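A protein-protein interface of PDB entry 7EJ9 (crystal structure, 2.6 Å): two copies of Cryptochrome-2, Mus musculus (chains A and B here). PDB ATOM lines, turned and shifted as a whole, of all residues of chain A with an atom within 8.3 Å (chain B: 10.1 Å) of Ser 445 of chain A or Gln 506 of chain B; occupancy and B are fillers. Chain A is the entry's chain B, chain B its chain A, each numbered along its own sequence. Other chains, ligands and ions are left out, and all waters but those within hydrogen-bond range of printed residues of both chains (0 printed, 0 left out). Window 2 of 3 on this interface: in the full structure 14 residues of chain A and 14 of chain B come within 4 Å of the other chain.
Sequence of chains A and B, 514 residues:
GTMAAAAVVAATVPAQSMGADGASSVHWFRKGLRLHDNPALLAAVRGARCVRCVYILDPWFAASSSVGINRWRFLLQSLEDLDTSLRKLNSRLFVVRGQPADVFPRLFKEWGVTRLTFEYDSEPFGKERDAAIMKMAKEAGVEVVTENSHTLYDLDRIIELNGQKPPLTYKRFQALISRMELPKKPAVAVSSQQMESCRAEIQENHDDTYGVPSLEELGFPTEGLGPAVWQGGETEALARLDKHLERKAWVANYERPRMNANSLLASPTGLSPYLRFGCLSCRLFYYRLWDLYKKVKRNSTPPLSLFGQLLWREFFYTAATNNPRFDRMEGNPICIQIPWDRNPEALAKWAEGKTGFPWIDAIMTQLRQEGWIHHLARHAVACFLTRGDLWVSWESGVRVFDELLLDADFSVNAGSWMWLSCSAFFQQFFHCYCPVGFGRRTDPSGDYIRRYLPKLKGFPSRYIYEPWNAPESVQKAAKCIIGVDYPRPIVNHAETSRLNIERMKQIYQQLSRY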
ATOM      1  N   ASN A 262      31.304  22.509   4.379  1.00  0.00           N
ATOM      2  CA  ASN A 262      30.319  23.421   4.952  1.00  0.00           C
ATOM      3  C   ASN A 262      29.911  22.968   6.354  1.00  0.00           C
ATOM      4  O   ASN A 262      29.366  23.751   7.136  1.00  0.00           O
ATOM      5  CB  ASN A 262      29.091  23.525   4.046  1.00  0.00           C
ATOM      6  N   SER A 263      30.174  21.696   6.658  1.00  0.00           N
ATOM      7  CA  SER A 263      29.966  21.133   7.983  1.00  0.00           C
ATOM      8  C   SER A 263      31.310  20.704   8.553  1.00  0.00           C
ATOM      9  O   SER A 263      32.266  20.446   7.814  1.00  0.00           O
ATOM     10  CB  SER A 263      29.002  19.931   7.953  1.00  0.00           C
ATOM     11  N   GLY A 439      34.205  29.625  17.033  1.00  0.00           N
ATOM     12  CA  GLY A 439      33.450  28.408  17.244  1.00  0.00           C
ATOM     13  C   GLY A 439      31.971  28.679  17.417  1.00  0.00           C
ATOM     14  O   GLY A 439      31.136  27.958  16.863  1.00  0.00           O
ATOM     15  N   ARG A 440      31.634  29.713  18.192  1.00  0.00           N
ATOM     16  CA  ARG A 440      30.234  30.090  18.352  1.00  0.00           C
ATOM     17  C   ARG A 440      29.609  30.468  17.014  1.00  0.00           C
ATOM     18  O   ARG A 440      28.446  30.146  16.752  1.00  0.00           O
ATOM     19  CB  ARG A 440      30.108  31.243  19.347  1.00  0.00           C
ATOM     20  N   ARG A 441      30.364  31.154  16.152  1.00  0.00           N
ATOM     21  CA  ARG A 441      29.817  31.548  14.858  1.00  0.00           C
ATOM     22  C   ARG A 441      29.753  30.364  13.900  1.00  0.00           C
ATOM     23  O   ARG A 441      28.802  30.241  13.118  1.00  0.00           O
ATOM     24  CB  ARG A 441      30.644  32.685  14.258  1.00  0.00           C
ATOM     25  N   THR A 442      30.751  29.479  13.951  1.00  0.00           N
ATOM     26  CA  THR A 442      30.762  28.321  13.063  1.00  0.00           C
ATOM     27  C   THR A 442      29.665  27.326  13.429  1.00  0.00           C
ATOM     28  O   THR A 442      29.021  26.754  12.544  1.00  0.00           O
ATOM     29  CB  THR A 442      32.131  27.647  13.103  1.00  0.00           C
ATOM     30  OG1 THR A 442      33.145  28.617  12.820  1.00  0.00           O
ATOM     31  CG2 THR A 442      32.212  26.532  12.081  1.00  0.00           C
ATOM     32  N   ASP A 443      29.442  27.105  14.726  1.00  0.00           N
ATOM     33  CA  ASP A 443      28.453  26.136  15.200  1.00  0.00           C
ATOM     34  C   ASP A 443      27.753  26.696  16.429  1.00  0.00           C
ATOM     35  O   ASP A 443      28.148  26.413  17.568  1.00  0.00           O
ATOM     36  CB  ASP A 443      29.104  24.790  15.515  1.00  0.00           C
ATOM     37  CG  ASP A 443      28.111  23.768  16.032  1.00  0.00           C
ATOM     38  OD1 ASP A 443      26.918  23.860  15.673  1.00  0.00           O
ATOM     39  OD2 ASP A 443      28.528  22.881  16.807  1.00  0.00           O
ATOM     40  N   PRO A 444      26.703  27.498  16.236  1.00  0.00           N
ATOM     41  CA  PRO A 444      25.965  28.026  17.395  1.00  0.00           C
ATOM     42  C   PRO A 444      25.384  26.946  18.287  1.00  0.00           C
ATOM     43  O   PRO A 444      25.148  27.204  19.473  1.00  0.00           O
ATOM     44  CB  PRO A 444      24.858  28.872  16.749  1.00  0.00           C
ATOM     45  CG  PRO A 444      25.381  29.215  15.397  1.00  0.00           C
ATOM     46  CD  PRO A 444      26.189  28.030  14.963  1.00  0.00           C
ATOM     47  N   SER A 445      25.145  25.745  17.754  1.00  0.00           N
ATOM     48  CA  SER A 445      24.574  24.676  18.568  1.00  0.00           C
ATOM     49  C   SER A 445      25.576  24.155  19.590  1.00  0.00           C
ATOM     50  O   SER A 445      25.197  23.773  20.704  1.00  0.00           O
ATOM     51  CB  SER A 445      24.090  23.537  17.674  1.00  0.00           C
ATOM     52  OG  SER A 445      25.177  22.875  17.058  1.00  0.00           O
ATOM     53  N   GLY A 446      26.861  24.137  19.236  1.00  0.00           N
ATOM     54  CA  GLY A 446      27.842  23.494  20.083  1.00  0.00           C
ATOM     55  C   GLY A 446      27.753  21.986  20.128  1.00  0.00           C
ATOM     56  O   GLY A 446      28.426  21.366  20.957  1.00  0.00           O
ATOM     57  N   ASP A 447      26.920  21.373  19.279  1.00  0.00           N
ATOM     58  CA  ASP A 447      26.871  19.915  19.236  1.00  0.00           C
ATOM     59  C   ASP A 447      28.193  19.338  18.762  1.00  0.00           C
ATOM     60  O   ASP A 447      28.505  18.182  19.063  1.00  0.00           O
ATOM     61  CB  ASP A 447      25.738  19.432  18.327  1.00  0.00           C
ATOM     62  CG  ASP A 447      24.377  19.892  18.793  1.00  0.00           C
ATOM     63  OD1 ASP A 447      24.198  20.065  20.017  1.00  0.00           O
ATOM     64  OD2 ASP A 447      23.488  20.073  17.937  1.00  0.00           O
ATOM     65  N   TYR A 448      28.967  20.118  18.001  1.00  0.00           N
ATOM     66  CA  TYR A 448      30.299  19.682  17.599  1.00  0.00           C
ATOM     67  C   TYR A 448      31.222  19.572  18.808  1.00  0.00           C
ATOM     68  O   TYR A 448      32.034  18.642  18.898  1.00  0.00           O
ATOM     69  CB  TYR A 448      30.869  20.651  16.561  1.00  0.00           C
ATOM     70  CG  TYR A 448      32.309  20.383  16.188  1.00  0.00           C
ATOM     71  CD1 TYR A 448      32.630  19.403  15.254  1.00  0.00           C
ATOM     72  CD2 TYR A 448      33.345  21.112  16.764  1.00  0.00           C
ATOM     73  CE1 TYR A 448      33.943  19.152  14.909  1.00  0.00           C
ATOM     74  CE2 TYR A 448      34.663  20.869  16.427  1.00  0.00           C
ATOM     75  CZ  TYR A 448      34.958  19.889  15.498  1.00  0.00           C
ATOM     76  OH  TYR A 448      36.269  19.638  15.153  1.00  0.00           O
ATOM     77  N   ILE A 449      31.108  20.513  19.748  1.00  0.00           N
ATOM     78  CA  ILE A 449      31.834  20.400  21.007  1.00  0.00           C
ATOM     79  C   ILE A 449      31.366  19.170  21.773  1.00  0.00           C
ATOM     80  O   ILE A 449      32.175  18.403  22.304  1.00  0.00           O
ATOM     81  CB  ILE A 449      31.662  21.681  21.842  1.00  0.00           C
ATOM     82  CG1 ILE A 449      31.952  22.924  20.993  1.00  0.00           C
ATOM     83  CG2 ILE A 449      32.565  21.639  23.071  1.00  0.00           C
ATOM     84  CD1 ILE A 449      33.368  22.988  20.462  1.00  0.00           C
ATOM     85  N   ARG A 450      30.047  18.957  21.829  1.00  0.00           N
ATOM     86  CA  ARG A 450      29.513  17.841  22.604  1.00  0.00           C
ATOM     87  C   ARG A 450      29.848  16.500  21.970  1.00  0.00           C
ATOM     88  O   ARG A 450      29.933  15.488  22.677  1.00  0.00           O
ATOM     89  CB  ARG A 450      28.001  17.983  22.757  1.00  0.00           C
ATOM     90  CG  ARG A 450      27.569  19.274  23.415  1.00  0.00           C
ATOM     91  CD  ARG A 450      26.082  19.284  23.753  1.00  0.00           C
ATOM     92  NE  ARG A 450      25.691  20.538  24.387  1.00  0.00           N
ATOM     93  CZ  ARG A 450      25.306  21.617  23.721  1.00  0.00           C
ATOM     94  NH1 ARG A 450      25.206  21.613  22.403  1.00  0.00           N
ATOM     95  NH2 ARG A 450      25.024  22.729  24.394  1.00  0.00           N
ATOM     96  N   LYS A 457      29.098  18.064  27.650  1.00  0.00           N
ATOM     97  CA  LYS A 457      27.761  17.912  27.081  1.00  0.00           C
ATOM     98  C   LYS A 457      26.706  18.628  27.911  1.00  0.00           C
ATOM     99  O   LYS A 457      25.695  19.082  27.365  1.00  0.00           O
ATOM    100  CB  LYS A 457      27.407  16.429  26.951  1.00  0.00           C
ATOM    101  N   PHE A 459      26.746  21.523  29.460  1.00  0.00           N
ATOM    102  CA  PHE A 459      26.688  22.978  29.416  1.00  0.00           C
ATOM    103  C   PHE A 459      25.690  23.456  28.360  1.00  0.00           C
ATOM    104  O   PHE A 459      25.527  22.823  27.311  1.00  0.00           O
ATOM    105  CB  PHE A 459      28.067  23.561  29.123  1.00  0.00           C
ATOM    106  CG  PHE A 459      29.017  23.475  30.278  1.00  0.00           C
ATOM    107  CD1 PHE A 459      29.148  24.533  31.164  1.00  0.00           C
ATOM    108  CD2 PHE A 459      29.780  22.338  30.479  1.00  0.00           C
ATOM    109  CE1 PHE A 459      30.023  24.456  32.227  1.00  0.00           C
ATOM    110  CE2 PHE A 459      30.655  22.255  31.542  1.00  0.00           C
ATOM    111  CZ  PHE A 459      30.777  23.316  32.417  1.00  0.00           C
ATOM    112  N   PRO A 460      25.005  24.566  28.616  1.00  0.00           N
ATOM    113  CA  PRO A 460      24.131  25.149  27.594  1.00  0.00           C
ATOM    114  C   PRO A 460      24.957  25.836  26.519  1.00  0.00           C
ATOM    115  O   PRO A 460      26.143  26.120  26.691  1.00  0.00           O
ATOM    116  CB  PRO A 460      23.289  26.150  28.379  1.00  0.00           C
ATOM    117  CG  PRO A 460      24.197  26.585  29.489  1.00  0.00           C
ATOM    118  CD  PRO A 460      25.025  25.371  29.850  1.00  0.00           C
ATOM    119  N   SER A 461      24.291  26.132  25.399  1.00  0.00           N
ATOM    120  CA  SER A 461      25.000  26.629  24.223  1.00  0.00           C
ATOM    121  C   SER A 461      25.673  27.976  24.470  1.00  0.00           C
ATOM    122  O   SER A 461      26.690  28.283  23.835  1.00  0.00           O
ATOM    123  CB  SER A 461      24.038  26.723  23.038  1.00  0.00           C
ATOM    124  OG  SER A 461      23.677  25.432  22.579  1.00  0.00           O
ATOM    125  N   ARG A 462      25.135  28.791  25.380  1.00  0.00           N
ATOM    126  CA  ARG A 462      25.732  30.097  25.640  1.00  0.00           C
ATOM    127  C   ARG A 462      27.028  29.997  26.437  1.00  0.00           C
ATOM    128  O   ARG A 462      27.767  30.984  26.519  1.00  0.00           O
ATOM    129  CB  ARG A 462      24.736  30.996  26.375  1.00  0.00           C
ATOM    130  N   ILE A 464      29.068  26.755  26.371  1.00  0.00           N
ATOM    131  CA  ILE A 464      29.891  25.608  26.016  1.00  0.00           C
ATOM    132  C   ILE A 464      31.188  26.020  25.329  1.00  0.00           C
ATOM    133  O   ILE A 464      32.163  25.263  25.364  1.00  0.00           O
ATOM    134  CB  ILE A 464      29.089  24.622  25.148  1.00  0.00           C
ATOM    135  CG1 ILE A 464      29.807  23.274  25.090  1.00  0.00           C
ATOM    136  CG2 ILE A 464      28.873  25.182  23.751  1.00  0.00           C
ATOM    137  CD1 ILE A 464      28.957  22.160  24.586  1.00  0.00           C
ATOM    138  N   TYR A 465      31.242  27.200  24.712  1.00  0.00           N
ATOM    139  CA  TYR A 465      32.502  27.680  24.157  1.00  0.00           C
ATOM    140  C   TYR A 465      33.326  28.452  25.170  1.00  0.00           C
ATOM    141  O   TYR A 465      34.529  28.641  24.957  1.00  0.00           O
ATOM    142  CB  TYR A 465      32.256  28.553  22.923  1.00  0.00           C
ATOM    143  CG  TYR A 465      31.814  27.747  21.731  1.00  0.00           C
ATOM    144  CD1 TYR A 465      32.735  27.057  20.956  1.00  0.00           C
ATOM    145  CD2 TYR A 465      30.475  27.659  21.392  1.00  0.00           C
ATOM    146  CE1 TYR A 465      32.333  26.307  19.872  1.00  0.00           C
ATOM    147  CE2 TYR A 465      30.065  26.914  20.309  1.00  0.00           C
ATOM    148  CZ  TYR A 465      30.995  26.239  19.554  1.00  0.00           C
ATOM    149  OH  TYR A 465      30.589  25.495  18.476  1.00  0.00           O
ATOM    150  N   ILE B 336      23.119  13.113   4.987  1.00  0.00           N
ATOM    151  CA  ILE B 336      23.650  14.321   5.601  1.00  0.00           C
ATOM    152  C   ILE B 336      24.240  13.964   6.954  1.00  0.00           C
ATOM    153  O   ILE B 336      23.640  13.210   7.730  1.00  0.00           O
ATOM    154  CB  ILE B 336      22.553  15.390   5.733  1.00  0.00           C
ATOM    155  CG1 ILE B 336      22.200  15.963   4.363  1.00  0.00           C
ATOM    156  CG2 ILE B 336      22.976  16.495   6.685  1.00  0.00           C
ATOM    157  CD1 ILE B 336      20.973  16.856   4.393  1.00  0.00           C
ATOM    158  N   GLN B 337      25.426  14.494   7.236  1.00  0.00           N
ATOM    159  CA  GLN B 337      26.142  14.183   8.466  1.00  0.00           C
ATOM    160  C   GLN B 337      25.746  15.184   9.546  1.00  0.00           C
ATOM    161  O   GLN B 337      26.011  16.383   9.414  1.00  0.00           O
ATOM    162  CB  GLN B 337      27.648  14.191   8.214  1.00  0.00           C
ATOM    163  CG  GLN B 337      28.059  13.323   7.032  1.00  0.00           C
ATOM    164  CD  GLN B 337      27.791  11.852   7.273  1.00  0.00           C
ATOM    165  OE1 GLN B 337      28.307  11.272   8.228  1.00  0.00           O
ATOM    166  NE2 GLN B 337      26.972  11.240   6.422  1.00  0.00           N
ATOM    167  N   ILE B 338      25.120  14.686  10.610  1.00  0.00           N
ATOM    168  CA  ILE B 338      24.492  15.500  11.648  1.00  0.00           C
ATOM    169  C   ILE B 338      24.988  15.007  13.001  1.00  0.00           C
ATOM    170  O   ILE B 338      24.998  13.789  13.243  1.00  0.00           O
ATOM    171  CB  ILE B 338      22.958  15.422  11.556  1.00  0.00           C
ATOM    172  CG1 ILE B 338      22.468  16.021  10.239  1.00  0.00           C
ATOM    173  CG2 ILE B 338      22.295  16.102  12.747  1.00  0.00           C
ATOM    174  CD1 ILE B 338      21.023  15.696   9.929  1.00  0.00           C
ATOM    175  N   PRO B 339      25.402  15.895  13.908  1.00  0.00           N
ATOM    176  CA  PRO B 339      25.899  15.422  15.214  1.00  0.00           C
ATOM    177  C   PRO B 339      24.751  15.057  16.147  1.00  0.00           C
ATOM    178  O   PRO B 339      24.283  15.843  16.968  1.00  0.00           O
ATOM    179  CB  PRO B 339      26.703  16.621  15.731  1.00  0.00           C
ATOM    180  CG  PRO B 339      26.419  17.767  14.782  1.00  0.00           C
ATOM    181  CD  PRO B 339      25.311  17.355  13.873  1.00  0.00           C
ATOM    182  N   TRP B 340      24.272  13.826  16.003  1.00  0.00           N
ATOM    183  CA  TRP B 340      23.159  13.357  16.816  1.00  0.00           C
ATOM    184  C   TRP B 340      23.607  13.161  18.256  1.00  0.00           C
ATOM    185  O   TRP B 340      24.746  12.767  18.517  1.00  0.00           O
ATOM    186  CB  TRP B 340      22.607  12.045  16.254  1.00  0.00           C
ATOM    187  CG  TRP B 340      22.077  12.177  14.861  1.00  0.00           C
ATOM    188  CD1 TRP B 340      22.601  11.624  13.729  1.00  0.00           C
ATOM    189  CD2 TRP B 340      20.921  12.917  14.447  1.00  0.00           C
ATOM    190  NE1 TRP B 340      21.843  11.969  12.641  1.00  0.00           N
ATOM    191  CE2 TRP B 340      20.807  12.764  13.052  1.00  0.00           C
ATOM    192  CE3 TRP B 340      19.974  13.696  15.121  1.00  0.00           C
ATOM    193  CZ2 TRP B 340      19.780  13.358  12.315  1.00  0.00           C
ATOM    194  CZ3 TRP B 340      18.954  14.284  14.389  1.00  0.00           C
ATOM    195  CH2 TRP B 340      18.866  14.110  13.001  1.00  0.00           C
ATOM    196  N   ASP B 341      22.706  13.458  19.192  1.00  0.00           N
ATOM    197  CA  ASP B 341      22.986  13.201  20.596  1.00  0.00           C
ATOM    198  C   ASP B 341      23.192  11.711  20.822  1.00  0.00           C
ATOM    199  O   ASP B 341      22.599  10.870  20.143  1.00  0.00           O
ATOM    200  CB  ASP B 341      21.841  13.698  21.483  1.00  0.00           C
ATOM    201  CG  ASP B 341      21.898  15.193  21.739  1.00  0.00           C
ATOM    202  OD1 ASP B 341      22.770  15.877  21.162  1.00  0.00           O
ATOM    203  OD2 ASP B 341      21.070  15.688  22.531  1.00  0.00           O
ATOM    204  N   TRP B 391      16.655  14.077  19.474  1.00  0.00           N
ATOM    205  CA  TRP B 391      17.830  14.325  18.636  1.00  0.00           C
ATOM    206  C   TRP B 391      18.768  13.121  18.608  1.00  0.00           C
ATOM    207  O   TRP B 391      19.984  13.264  18.437  1.00  0.00           O
ATOM    208  CB  TRP B 391      18.586  15.581  19.085  1.00  0.00           C
ATOM    209  CG  TRP B 391      19.375  16.208  17.988  1.00  0.00           C
ATOM    210  CD1 TRP B 391      20.729  16.164  17.819  1.00  0.00           C
ATOM    211  CD2 TRP B 391      18.856  16.966  16.890  1.00  0.00           C
ATOM    212  NE1 TRP B 391      21.086  16.856  16.684  1.00  0.00           N
ATOM    213  CE2 TRP B 391      19.954  17.357  16.097  1.00  0.00           C
ATOM    214  CE3 TRP B 391      17.571  17.357  16.502  1.00  0.00           C
ATOM    215  CZ2 TRP B 391      19.803  18.118  14.939  1.00  0.00           C
ATOM    216  CZ3 TRP B 391      17.425  18.111  15.353  1.00  0.00           C
ATOM    217  CH2 TRP B 391      18.535  18.483  14.585  1.00  0.00           C
ATOM    218  N   ARG B 498      12.351  23.839  20.587  1.00  0.00           N
ATOM    219  CA  ARG B 498      13.043  25.105  20.359  1.00  0.00           C
ATOM    220  C   ARG B 498      14.512  24.869  20.026  1.00  0.00           C
ATOM    221  O   ARG B 498      15.029  25.394  19.030  1.00  0.00           O
ATOM    222  CB  ARG B 498      12.905  26.009  21.586  1.00  0.00           C
ATOM    223  N   LEU B 499      15.199  24.074  20.850  1.00  0.00           N
ATOM    224  CA  LEU B 499      16.580  23.706  20.556  1.00  0.00           C
ATOM    225  C   LEU B 499      16.679  22.990  19.216  1.00  0.00           C
ATOM    226  O   LEU B 499      17.544  23.304  18.391  1.00  0.00           O
ATOM    227  CB  LEU B 499      17.136  22.824  21.675  1.00  0.00           C
ATOM    228  CG  LEU B 499      16.998  23.349  23.107  1.00  0.00           C
ATOM    229  CD1 LEU B 499      17.309  22.253  24.116  1.00  0.00           C
ATOM    230  CD2 LEU B 499      17.890  24.564  23.339  1.00  0.00           C
ATOM    231  N   ASN B 500      15.781  22.030  18.975  1.00  0.00           N
ATOM    232  CA  ASN B 500      15.878  21.206  17.776  1.00  0.00           C
ATOM    233  C   ASN B 500      15.551  22.000  16.517  1.00  0.00           C
ATOM    234  O   ASN B 500      16.136  21.755  15.456  1.00  0.00           O
ATOM    235  CB  ASN B 500      14.955  19.993  17.897  1.00  0.00           C
ATOM    236  CG  ASN B 500      15.462  18.970  18.895  1.00  0.00           C
ATOM    237  OD1 ASN B 500      16.522  19.144  19.493  1.00  0.00           O
ATOM    238  ND2 ASN B 500      14.700  17.902  19.088  1.00  0.00           N
ATOM    239  N   ILE B 501      14.614  22.946  16.606  1.00  0.00           N
ATOM    240  CA  ILE B 501      14.260  23.735  15.428  1.00  0.00           C
ATOM    241  C   ILE B 501      15.434  24.603  14.994  1.00  0.00           C
ATOM    242  O   ILE B 501      15.723  24.725  13.798  1.00  0.00           O
ATOM    243  CB  ILE B 501      12.995  24.573  15.693  1.00  0.00           C
ATOM    244  CG1 ILE B 501      11.750  23.683  15.647  1.00  0.00           C
ATOM    245  CG2 ILE B 501      12.861  25.692  14.672  1.00  0.00           C
ATOM    246  CD1 ILE B 501      10.515  24.331  16.221  1.00  0.00           C
ATOM    247  N   GLU B 502      16.136  25.210  15.953  1.00  0.00           N
ATOM    248  CA  GLU B 502      17.306  26.009  15.606  1.00  0.00           C
ATOM    249  C   GLU B 502      18.431  25.137  15.057  1.00  0.00           C
ATOM    250  O   GLU B 502      19.154  25.555  14.145  1.00  0.00           O
ATOM    251  CB  GLU B 502      17.774  26.808  16.821  1.00  0.00           C
ATOM    252  CG  GLU B 502      16.823  27.926  17.219  1.00  0.00           C
ATOM    253  CD  GLU B 502      17.245  28.620  18.500  1.00  0.00           C
ATOM    254  OE1 GLU B 502      18.271  28.212  19.085  1.00  0.00           O
ATOM    255  OE2 GLU B 502      16.553  29.571  18.923  1.00  0.00           O
ATOM    256  N   ARG B 503      18.595  23.924  15.594  1.00  0.00           N
ATOM    257  CA  ARG B 503      19.547  22.981  15.009  1.00  0.00           C
ATOM    258  C   ARG B 503      19.208  22.694  13.552  1.00  0.00           C
ATOM    259  O   ARG B 503      20.093  22.676  12.689  1.00  0.00           O
ATOM    260  CB  ARG B 503      19.559  21.675  15.797  1.00  0.00           C
ATOM    261  CG  ARG B 503      20.182  21.746  17.163  1.00  0.00           C
ATOM    262  CD  ARG B 503      19.668  20.591  17.988  1.00  0.00           C
ATOM    263  NE  ARG B 503      20.713  19.997  18.806  1.00  0.00           N
ATOM    264  CZ  ARG B 503      20.486  19.162  19.808  1.00  0.00           C
ATOM    265  NH1 ARG B 503      19.257  18.819  20.157  1.00  0.00           N
ATOM    266  NH2 ARG B 503      21.517  18.663  20.481  1.00  0.00           N
ATOM    267  N   MET B 504      17.929  22.450  13.267  1.00  0.00           N
ATOM    268  CA  MET B 504      17.506  22.182  11.898  1.00  0.00           C
ATOM    269  C   MET B 504      17.693  23.401  11.003  1.00  0.00           C
ATOM    270  O   MET B 504      17.987  23.250   9.811  1.00  0.00           O
ATOM    271  CB  MET B 504      16.048  21.720  11.886  1.00  0.00           C
ATOM    272  CG  MET B 504      15.880  20.224  12.102  1.00  0.00           C
ATOM    273  SD  MET B 504      16.451  19.305  10.662  1.00  0.00           S
ATOM    274  CE  MET B 504      17.116  17.830  11.432  1.00  0.00           C
ATOM    275  N   LYS B 505      17.523  24.608  11.550  1.00  0.00           N
ATOM    276  CA  LYS B 505      17.759  25.809  10.758  1.00  0.00           C
ATOM    277  C   LYS B 505      19.228  25.917  10.359  1.00  0.00           C
ATOM    278  O   LYS B 505      19.547  26.340   9.241  1.00  0.00           O
ATOM    279  CB  LYS B 505      17.307  27.045  11.535  1.00  0.00           C
ATOM    280  N   GLN B 506      20.134  25.518  11.256  1.00  0.00           N
ATOM    281  CA  GLN B 506      21.557  25.505  10.929  1.00  0.00           C
ATOM    282  C   GLN B 506      21.850  24.545   9.784  1.00  0.00           C
ATOM    283  O   GLN B 506      22.491  24.920   8.795  1.00  0.00           O
ATOM    284  CB  GLN B 506      22.380  25.117  12.159  1.00  0.00           C
ATOM    285  CG  GLN B 506      22.453  26.176  13.241  1.00  0.00           C
ATOM    286  CD  GLN B 506      23.230  25.698  14.455  1.00  0.00           C
ATOM    287  OE1 GLN B 506      22.728  25.739  15.581  1.00  0.00           O
ATOM    288  NE2 GLN B 506      24.457  25.233  14.231  1.00  0.00           N
ATOM    289  N   ILE B 507      21.399  23.292   9.909  1.00  0.00           N
ATOM    290  CA  ILE B 507      21.702  22.283   8.898  1.00  0.00           C
ATOM    291  C   ILE B 507      21.163  22.712   7.541  1.00  0.00           C
ATOM    292  O   ILE B 507      21.842  22.577   6.516  1.00  0.00           O
ATOM    293  CB  ILE B 507      21.146  20.912   9.324  1.00  0.00           C
ATOM    294  N   TYR B 508      19.947  23.249   7.514  1.00  0.00           N
ATOM    295  CA  TYR B 508      19.364  23.768   6.283  1.00  0.00           C
ATOM    296  C   TYR B 508      19.515  25.291   6.209  1.00  0.00           C
ATOM    297  O   TYR B 508      20.617  25.814   6.008  1.00  0.00           O
ATOM    298  CB  TYR B 508      17.887  23.370   6.182  1.00  0.00           C
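The side-chain carboxylate (OD1) of Asp 447 of chain A is in salt-bridge range of the guanidinium group (NH1) of Arg 450 of chain A (3.0 Å).
The guanidinium group (NH1) of Arg 450 of chain A lies within hydrogen-bond range of the backbone carbonyl oxygen (O) of Ser 445 of chain A.
OD1 of Asp 341 of chain B is in salt-bridge range of NH2 of Arg 503 of chain B, 3.1 Å away.
The side-chain amide oxygen (OD1) of Asn 500 of chain B lies within hydrogen-bond range of the guanidinium group (NH1) of Arg 503 of chain B.
The backbone NH (N) of Tyr 448 of chain A sits at hydrogen-bond distance from the side-chain carboxylate (OD2) of Asp 443 of chain A (3.0 Å).
The backbone carbonyl oxygen (O) of Asp 443 of chain A lies within hydrogen-bond range of the side-chain hydroxyl (OH) of Tyr 465 of chain A (2.8 Å).
Of the 18 printed residues of chain B, 3 touch a printed residue of chain A.
Hydrophobic or aromatic side chains of chain B within 4 Å of the printed part of chain A: Pro 339.
Hydrophobic or aromatic side chains of chain A that line the printed part of chain B: Pro 444.
Along chain A the printed residues that touch a printed residue of chain B span positions 443 to 447.
Among the printed residues, 5 pairs touch across the chains.
No position is printed for both chains.
Arg 441 of chain A touches none of the printed residues of chain B.
Of chain B, only Gln 506 (3.2 Å) comes within 4 Å of Asp 443 of chain A.
Of chain B, only Gln 506 comes within 4 Å of Pro 444 of chain A.
Printed residues of chain B within 4 Å of Asp 447 of chain A: Pro 339 (3.9 Å) and Arg 503 (2.9 Å).
No residue of chain B comes within 4 Å of Ser 461 of chain A.
Tyr 465 of chain A touches none of the printed residues of chain B.
Of the printed residues of chain A, Pro 339 of chain B touches Asp 447 (3.9 Å).
Of the printed residues of chain A, Arg 503 of chain B touches Asp 447 (2.9 Å).
No residue of chain A comes within 4 Å of Ile 507 of chain B.
The nearest residue of chain B that does not touch Ser 445 of chain A is Arg 503 of chain B (4.3 Å).
The nearest residue of chain A that does not touch Gln 506 of chain B is Thr 442 of chain A (5.1 Å).
The nearest printed residue of chain A that does not touch Arg 503 of chain B is Ser 445 of chain A (4.3 Å).
OD2 of Asp 447 of chain A lies within salt-bridge range of NE of Arg 503 of chain B (2.9 Å).
The side-chain amide nitrogen (NE2) of Gln 506 of chain B lies within hydrogen-bond range of the side-chain carboxylate (OD1) of Asp 443 of chain A, at 3.2 Å.
The backbone NH (N) of Ser 445 of chain A lies within hydrogen-bond range of the side-chain amide oxygen (OE1) of Gln 506 of chain B (3.3 Å).
Gln 506 of chain B touches Pro 444 of chain A (NE2 to CD, 3.4 Å).
Asp 447 of chain A touches Pro 339 of chain B (CB to CB, 3.9 Å).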
